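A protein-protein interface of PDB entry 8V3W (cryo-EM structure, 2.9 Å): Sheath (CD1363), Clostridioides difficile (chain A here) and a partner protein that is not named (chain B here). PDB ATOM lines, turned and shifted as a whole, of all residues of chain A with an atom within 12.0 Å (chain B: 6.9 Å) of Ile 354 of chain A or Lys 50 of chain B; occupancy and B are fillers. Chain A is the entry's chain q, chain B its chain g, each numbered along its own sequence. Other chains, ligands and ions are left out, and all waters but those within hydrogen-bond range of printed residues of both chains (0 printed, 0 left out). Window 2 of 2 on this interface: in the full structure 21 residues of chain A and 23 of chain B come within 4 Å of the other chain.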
ATOM      1  N   LEU A 350     -19.461  16.268  10.302  1.00  0.00           N
ATOM      2  CA  LEU A 350     -20.526  16.537  11.257  1.00  0.00           C
ATOM      3  C   LEU A 350     -20.108  16.072  12.643  1.00  0.00           C
ATOM      4  O   LEU A 350     -19.701  14.921  12.821  1.00  0.00           O
ATOM      5  CB  LEU A 350     -21.822  15.839  10.847  1.00  0.00           C
ATOM      6  CG  LEU A 350     -22.528  16.387   9.612  1.00  0.00           C
ATOM      7  CD1 LEU A 350     -23.786  15.598   9.333  1.00  0.00           C
ATOM      8  CD2 LEU A 350     -22.845  17.856   9.803  1.00  0.00           C
ATOM      9  N   SER A 351     -20.212  16.966  13.617  1.00  0.00           N
ATOM     10  CA  SER A 351     -20.007  16.637  15.022  1.00  0.00           C
ATOM     11  C   SER A 351     -21.360  16.734  15.713  1.00  0.00           C
ATOM     12  O   SER A 351     -21.875  17.834  15.928  1.00  0.00           O
ATOM     13  CB  SER A 351     -18.986  17.575  15.659  1.00  0.00           C
ATOM     14  OG  SER A 351     -19.107  17.575  17.067  1.00  0.00           O
ATOM     15  N   ILE A 352     -21.933  15.585  16.055  1.00  0.00           N
ATOM     16  CA  ILE A 352     -23.294  15.505  16.574  1.00  0.00           C
ATOM     17  C   ILE A 352     -23.230  15.268  18.073  1.00  0.00           C
ATOM     18  O   ILE A 352     -22.455  14.428  18.544  1.00  0.00           O
ATOM     19  CB  ILE A 352     -24.092  14.397  15.869  1.00  0.00           C
ATOM     20  CG1 ILE A 352     -24.157  14.672  14.367  1.00  0.00           C
ATOM     21  CG2 ILE A 352     -25.492  14.299  16.439  1.00  0.00           C
ATOM     22  CD1 ILE A 352     -24.926  13.644  13.593  1.00  0.00           C
ATOM     23  N   GLU A 353     -24.038  16.011  18.825  1.00  0.00           N
ATOM     24  CA  GLU A 353     -24.049  15.951  20.280  1.00  0.00           C
ATOM     25  C   GLU A 353     -25.323  15.259  20.747  1.00  0.00           C
ATOM     26  O   GLU A 353     -26.406  15.850  20.706  1.00  0.00           O
ATOM     27  CB  GLU A 353     -23.937  17.349  20.880  1.00  0.00           C
ATOM     28  CG  GLU A 353     -22.559  17.958  20.735  1.00  0.00           C
ATOM     29  CD  GLU A 353     -22.597  19.460  20.565  1.00  0.00           C
ATOM     30  OE1 GLU A 353     -23.006  20.156  21.515  1.00  0.00           O
ATOM     31  OE2 GLU A 353     -22.210  19.946  19.480  1.00  0.00           O
ATOM     32  N   ILE A 354     -25.181  14.009  21.183  1.00  0.00           N
ATOM     33  CA  ILE A 354     -26.250  13.260  21.835  1.00  0.00           C
ATOM     34  C   ILE A 354     -27.465  13.065  20.934  1.00  0.00           C
ATOM     35  O   ILE A 354     -27.990  11.956  20.818  1.00  0.00           O
ATOM     36  CB  ILE A 354     -26.653  13.945  23.149  1.00  0.00           C
ATOM     37  CG1 ILE A 354     -25.627  13.634  24.244  1.00  0.00           C
ATOM     38  CG2 ILE A 354     -28.055  13.536  23.565  1.00  0.00           C
ATOM     39  CD1 ILE A 354     -25.167  12.195  24.278  1.00  0.00           C
ATOM     40  N   PHE B  25     -36.926   3.058  23.520  1.00  0.00           N
ATOM     41  CA  PHE B  25     -36.330   2.875  22.203  1.00  0.00           C
ATOM     42  C   PHE B  25     -35.187   1.874  22.289  1.00  0.00           C
ATOM     43  O   PHE B  25     -34.258   2.051  23.081  1.00  0.00           O
ATOM     44  CB  PHE B  25     -35.834   4.215  21.663  1.00  0.00           C
ATOM     45  CG  PHE B  25     -35.578   4.220  20.184  1.00  0.00           C
ATOM     46  CD1 PHE B  25     -34.336   3.883  19.684  1.00  0.00           C
ATOM     47  CD2 PHE B  25     -36.577   4.569  19.297  1.00  0.00           C
ATOM     48  CE1 PHE B  25     -34.095   3.886  18.330  1.00  0.00           C
ATOM     49  CE2 PHE B  25     -36.342   4.575  17.942  1.00  0.00           C
ATOM     50  CZ  PHE B  25     -35.100   4.232  17.457  1.00  0.00           C
ATOM     51  N   ILE B  47     -28.910  -2.610  22.297  1.00  0.00           N
ATOM     52  CA  ILE B  47     -28.726  -1.460  23.171  1.00  0.00           C
ATOM     53  C   ILE B  47     -30.040  -0.686  23.222  1.00  0.00           C
ATOM     54  O   ILE B  47     -30.998  -1.002  22.519  1.00  0.00           O
ATOM     55  CB  ILE B  47     -27.563  -0.565  22.710  1.00  0.00           C
ATOM     56  CG1 ILE B  47     -27.786  -0.110  21.270  1.00  0.00           C
ATOM     57  CG2 ILE B  47     -26.246  -1.304  22.834  1.00  0.00           C
ATOM     58  CD1 ILE B  47     -26.609   0.603  20.671  1.00  0.00           C
ATOM     59  N   GLU B  48     -30.084   0.342  24.067  1.00  0.00           N
ATOM     60  CA  GLU B  48     -31.325   1.071  24.278  1.00  0.00           C
ATOM     61  C   GLU B  48     -31.062   2.558  24.477  1.00  0.00           C
ATOM     62  O   GLU B  48     -29.954   2.981  24.812  1.00  0.00           O
ATOM     63  CB  GLU B  48     -32.097   0.523  25.482  1.00  0.00           C
ATOM     64  CG  GLU B  48     -31.478   0.877  26.818  1.00  0.00           C
ATOM     65  CD  GLU B  48     -32.376   0.532  27.985  1.00  0.00           C
ATOM     66  OE1 GLU B  48     -33.519   0.089  27.748  1.00  0.00           O
ATOM     67  OE2 GLU B  48     -31.938   0.699  29.141  1.00  0.00           O
ATOM     68  N   LYS B  49     -32.120   3.341  24.262  1.00  0.00           N
ATOM     69  CA  LYS B  49     -32.169   4.785  24.519  1.00  0.00           C
ATOM     70  C   LYS B  49     -31.107   5.498  23.691  1.00  0.00           C
ATOM     71  O   LYS B  49     -31.119   5.362  22.456  1.00  0.00           O
ATOM     72  CB  LYS B  49     -32.102   5.036  26.026  1.00  0.00           C
ATOM     73  CG  LYS B  49     -33.280   4.490  26.805  1.00  0.00           C
ATOM     74  CD  LYS B  49     -33.100   4.728  28.291  1.00  0.00           C
ATOM     75  CE  LYS B  49     -34.285   4.211  29.081  1.00  0.00           C
ATOM     76  NZ  LYS B  49     -34.096   4.405  30.544  1.00  0.00           N
ATOM     77  N   LYS B  50     -30.190   6.250  24.303  1.00  0.00           N
ATOM     78  CA  LYS B  50     -29.402   7.239  23.575  1.00  0.00           C
ATOM     79  C   LYS B  50     -28.493   6.596  22.535  1.00  0.00           C
ATOM     80  O   LYS B  50     -28.299   7.147  21.447  1.00  0.00           O
ATOM     81  CB  LYS B  50     -28.602   8.072  24.568  1.00  0.00           C
ATOM     82  CG  LYS B  50     -28.265   9.458  24.087  1.00  0.00           C
ATOM     83  CD  LYS B  50     -28.031  10.378  25.269  1.00  0.00           C
ATOM     84  CE  LYS B  50     -29.225  10.369  26.204  1.00  0.00           C
ATOM     85  NZ  LYS B  50     -30.465  10.736  25.474  1.00  0.00           N
ATOM     86  N   GLU B  51     -27.914   5.438  22.852  1.00  0.00           N
ATOM     87  CA  GLU B  51     -27.043   4.765  21.894  1.00  0.00           C
ATOM     88  C   GLU B  51     -27.829   4.260  20.688  1.00  0.00           C
ATOM     89  O   GLU B  51     -27.359   4.346  19.542  1.00  0.00           O
ATOM     90  CB  GLU B  51     -26.317   3.621  22.594  1.00  0.00           C
ATOM     91  CG  GLU B  51     -25.830   3.982  23.985  1.00  0.00           C
ATOM     92  CD  GLU B  51     -24.808   5.100  23.974  1.00  0.00           C
ATOM     93  OE1 GLU B  51     -24.002   5.164  23.024  1.00  0.00           O
ATOM     94  OE2 GLU B  51     -24.811   5.922  24.914  1.00  0.00           O
ATOM     95  N   ALA B  52     -29.029   3.733  20.924  1.00  0.00           N
ATOM     96  CA  ALA B  52     -29.890   3.333  19.818  1.00  0.00           C
ATOM     97  C   ALA B  52     -30.249   4.529  18.946  1.00  0.00           C
ATOM     98  O   ALA B  52     -30.282   4.429  17.712  1.00  0.00           O
ATOM     99  CB  ALA B  52     -31.150   2.662  20.362  1.00  0.00           C
ATOM    100  N   LEU B  53     -30.526   5.671  19.575  1.00  0.00           N
ATOM    101  CA  LEU B  53     -30.806   6.883  18.818  1.00  0.00           C
ATOM    102  C   LEU B  53     -29.595   7.310  18.001  1.00  0.00           C
ATOM    103  O   LEU B  53     -29.740   7.801  16.878  1.00  0.00           O
ATOM    104  CB  LEU B  53     -31.248   7.996  19.762  1.00  0.00           C
ATOM    105  CG  LEU B  53     -32.710   7.897  20.189  1.00  0.00           C
ATOM    106  CD1 LEU B  53     -33.135   9.136  20.937  1.00  0.00           C
ATOM    107  CD2 LEU B  53     -33.590   7.685  18.979  1.00  0.00           C
ATOM    108  N   LYS B  54     -28.391   7.133  18.548  1.00  0.00           N
ATOM    109  CA  LYS B  54     -27.188   7.425  17.778  1.00  0.00           C
ATOM    110  C   LYS B  54     -27.114   6.556  16.532  1.00  0.00           C
ATOM    111  O   LYS B  54     -26.791   7.044  15.441  1.00  0.00           O
ATOM    112  CB  LYS B  54     -25.944   7.214  18.637  1.00  0.00           C
ATOM    113  CG  LYS B  54     -25.749   8.237  19.728  1.00  0.00           C
ATOM    114  CD  LYS B  54     -24.428   8.010  20.429  1.00  0.00           C
ATOM    115  CE  LYS B  54     -24.303   8.880  21.663  1.00  0.00           C
ATOM    116  NZ  LYS B  54     -22.957   8.754  22.280  1.00  0.00           N
ATOM    117  N   VAL B  55     -27.412   5.265  16.678  1.00  0.00           N
ATOM    118  CA  VAL B  55     -27.388   4.364  15.527  1.00  0.00           C
ATOM    119  C   VAL B  55     -28.398   4.812  14.476  1.00  0.00           C
ATOM    120  O   VAL B  55     -28.092   4.878  13.276  1.00  0.00           O
ATOM    121  CB  VAL B  55     -27.650   2.916  15.977  1.00  0.00           C
ATOM    122  CG1 VAL B  55     -27.861   2.021  14.776  1.00  0.00           C
ATOM    123  CG2 VAL B  55     -26.501   2.410  16.811  1.00  0.00           C
ATOM    124  N   ILE B  57     -29.683   7.801  13.999  1.00  0.00           N
ATOM    125  CA  ILE B  57     -29.275   9.074  13.414  1.00  0.00           C
ATOM    126  C   ILE B  57     -28.189   8.857  12.371  1.00  0.00           C
ATOM    127  O   ILE B  57     -28.220   9.451  11.285  1.00  0.00           O
ATOM    128  CB  ILE B  57     -28.810  10.031  14.524  1.00  0.00           C
ATOM    129  CG1 ILE B  57     -30.013  10.622  15.259  1.00  0.00           C
ATOM    130  CG2 ILE B  57     -27.930  11.124  13.962  1.00  0.00           C
ATOM    131  CD1 ILE B  57     -29.658  11.263  16.570  1.00  0.00           C
ATOM    132  N   VAL B 129     -24.111  19.925  15.454  1.00  0.00           N
ATOM    133  CA  VAL B 129     -25.533  19.616  15.517  1.00  0.00           C
ATOM    134  C   VAL B 129     -25.863  19.175  16.934  1.00  0.00           C
ATOM    135  O   VAL B 129     -25.165  18.327  17.500  1.00  0.00           O
ATOM    136  CB  VAL B 129     -25.920  18.525  14.504  1.00  0.00           C
ATOM    137  CG1 VAL B 129     -27.416  18.288  14.524  1.00  0.00           C
ATOM    138  CG2 VAL B 129     -25.457  18.903  13.118  1.00  0.00           C
ATOM    139  N   LYS B 130     -26.918  19.749  17.505  1.00  0.00           N
ATOM    140  CA  LYS B 130     -27.367  19.408  18.848  1.00  0.00           C
ATOM    141  C   LYS B 130     -28.776  18.842  18.773  1.00  0.00           C
ATOM    142  O   LYS B 130     -29.700  19.526  18.324  1.00  0.00           O
ATOM    143  CB  LYS B 130     -27.324  20.632  19.760  1.00  0.00           C
ATOM    144  CG  LYS B 130     -26.010  21.385  19.698  1.00  0.00           C
ATOM    145  CD  LYS B 130     -26.030  22.608  20.596  1.00  0.00           C
ATOM    146  CE  LYS B 130     -24.720  23.369  20.511  1.00  0.00           C
ATOM    147  NZ  LYS B 130     -23.569  22.503  20.884  1.00  0.00           N
ATOM    148  N   VAL B 131     -28.942  17.605  19.236  1.00  0.00           N
ATOM    149  CA  VAL B 131     -30.212  16.890  19.183  1.00  0.00           C
ATOM    150  C   VAL B 131     -30.748  16.752  20.599  1.00  0.00           C
ATOM    151  O   VAL B 131     -30.023  16.325  21.503  1.00  0.00           O
ATOM    152  CB  VAL B 131     -30.052  15.508  18.527  1.00  0.00           C
ATOM    153  CG1 VAL B 131     -31.401  14.945  18.144  1.00  0.00           C
ATOM    154  CG2 VAL B 131     -29.141  15.588  17.321  1.00  0.00           C
ATOM    155  N   SER B 132     -32.016  17.102  20.789  1.00  0.00           N
ATOM    156  CA  SER B 132     -32.688  16.979  22.078  1.00  0.00           C
ATOM    157  C   SER B 132     -33.755  15.897  21.984  1.00  0.00           C
ATOM    158  O   SER B 132     -34.630  15.960  21.116  1.00  0.00           O
ATOM    159  CB  SER B 132     -33.311  18.307  22.501  1.00  0.00           C
ATOM    160  OG  SER B 132     -32.352  19.347  22.472  1.00  0.00           O
ATOM    161  N   THR B 133     -33.686  14.920  22.881  1.00  0.00           N
ATOM    162  CA  THR B 133     -34.615  13.801  22.920  1.00  0.00           C
ATOM    163  C   THR B 133     -35.456  13.870  24.190  1.00  0.00           C
ATOM    164  O   THR B 133     -35.296  14.762  25.025  1.00  0.00           O
ATOM    165  CB  THR B 133     -33.861  12.474  22.839  1.00  0.00           C
ATOM    166  OG1 THR B 133     -33.452  12.081  24.153  1.00  0.00           O
ATOM    167  CG2 THR B 133     -32.633  12.620  21.966  1.00  0.00           C
ATOM    168  N   ILE B 134     -36.379  12.915  24.321  1.00  0.00           N
ATOM    169  CA  ILE B 134     -37.216  12.854  25.516  1.00  0.00           C
ATOM    170  C   ILE B 134     -36.404  12.397  26.722  1.00  0.00           C
ATOM    171  O   ILE B 134     -36.626  12.862  27.846  1.00  0.00           O
ATOM    172  CB  ILE B 134     -38.441  11.956  25.267  1.00  0.00           C
ATOM    173  CG1 ILE B 134     -38.013  10.564  24.807  1.00  0.00           C
ATOM    174  CG2 ILE B 134     -39.375  12.605  24.260  1.00  0.00           C
ATOM    175  CD1 ILE B 134     -39.108   9.793  24.115  1.00  0.00           C
ATOM    176  N   TYR B 135     -35.462  11.486  26.517  1.00  0.00           N
ATOM    177  CA  TYR B 135     -34.604  11.022  27.598  1.00  0.00           C
ATOM    178  C   TYR B 135     -33.581  12.081  27.985  1.00  0.00           C
ATOM    179  O   TYR B 135     -33.621  12.618  29.090  1.00  0.00           O
ATOM    180  CB  TYR B 135     -33.896   9.729  27.193  1.00  0.00           C
ATOM    181  CG  TYR B 135     -34.820   8.704  26.588  1.00  0.00           C
ATOM    182  CD1 TYR B 135     -35.724   8.012  27.378  1.00  0.00           C
ATOM    183  CD2 TYR B 135     -34.800   8.437  25.229  1.00  0.00           C
ATOM    184  CE1 TYR B 135     -36.575   7.075  26.832  1.00  0.00           C
ATOM    185  CE2 TYR B 135     -35.649   7.501  24.674  1.00  0.00           C
ATOM    186  CZ  TYR B 135     -36.535   6.823  25.481  1.00  0.00           C
ATOM    187  OH  TYR B 135     -37.385   5.889  24.941  1.00  0.00           O
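NZ of Lys 130 of chain B is in salt-bridge range of OE1 of Glu 353 of chain A (2.5 Å). The backbone NH (N) of Glu 353 of chain A sits at hydrogen-bond distance from the backbone carbonyl oxygen (O) of Val 129 of chain B, at 2.9 Å. N of Val 129 of chain B is in hydrogen-bond range of O of Ser 351 of chain A. O of Glu 353 of chain A lies within hydrogen-bond range of N of Val 131 of chain B, 3.4 Å away.
CD1 of Ile 352 of chain A touches CG2 of Ile 57 of chain B, at 3.9 Å. Ile 352 of chain A touches Val 129 of chain B. CG2 of Ile 352 of chain A touches CG2 of Val 131 of chain B, 3.97 Å away. CD1 of Ile 354 of chain A touches CD of Lys 50 of chain B, 3.5 Å away. Ile 354 of chain A touches Val 131 of chain B (CG2 to O, 3.99 Å).
Printed residues of chain A that touch a printed residue of chain B: Ser 351, Ile 352, Glu 353 and Ile 354. Along chain A the printed residues that touch a printed residue of chain B span positions 351 to 354. Hydrophobic or aromatic side chains of chain B that line the printed part of chain A: Ile 57 and Val 131. Among the printed residues, Asp or Glu carboxylates within 4 Å of a Lys or Arg side-chain nitrogen of the other chain: Glu 353 of chain A with Lys 130 of chain B (2.5 Å).
Of the printed residues of chain B, Ser 351 of chain A touches Val 129. Printed residues of chain B within 4 Å of Ile 352 of chain A: Ile 57 (3.9 Å), Val 129 (3.5 Å) and Val 131 (3.97 Å). Printed residues of chain B within 4 Å of Ile 354 of chain A: Lys 50 and Val 131. Phe 25 of chain B touches none of the printed residues of chain A. Ile 47 of chain B touches none of the printed residues of chain A. No residue of chain A comes within 4 Å of Glu 48 of chain B. No residue of chain A comes within 4 Å of Lys 49 of chain B. Lys 50 of chain B touches just one residue of chain A: Ile 354 (3.5 Å). No residue of chain A comes within 4 Å of Glu 51 of chain B. No residue of chain A comes within 4 Å of Ala 52 of chain B. No residue of chain A comes within 4 Å of Leu 53 of chain B. No residue of chain A comes within 4 Å of Lys 54 of chain B. Of the printed residues of chain A, Val 129 of chain B touches Ser 351 (3.1 Å), Ile 352 (3.5 Å) and Glu 353 (2.9 Å). Printed residues of chain A within 4 Å of Lys 130 of chain B: Glu 353. Of the printed residues of chain A, Val 131 of chain B touches Ile 352, Glu 353 and Ile 354. No residue of chain A comes within 4 Å of Ser 132 of chain B. No residue of chain A comes within 4 Å of Thr 133 of chain B. The nearest printed residue of chain B that does not touch Ile 354 of chain A is Lys 54 of chain B (4.3 Å). The nearest printed residue of chain A that does not touch Lys 130 of chain B is Ser 351 of chain A (5.6 Å).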
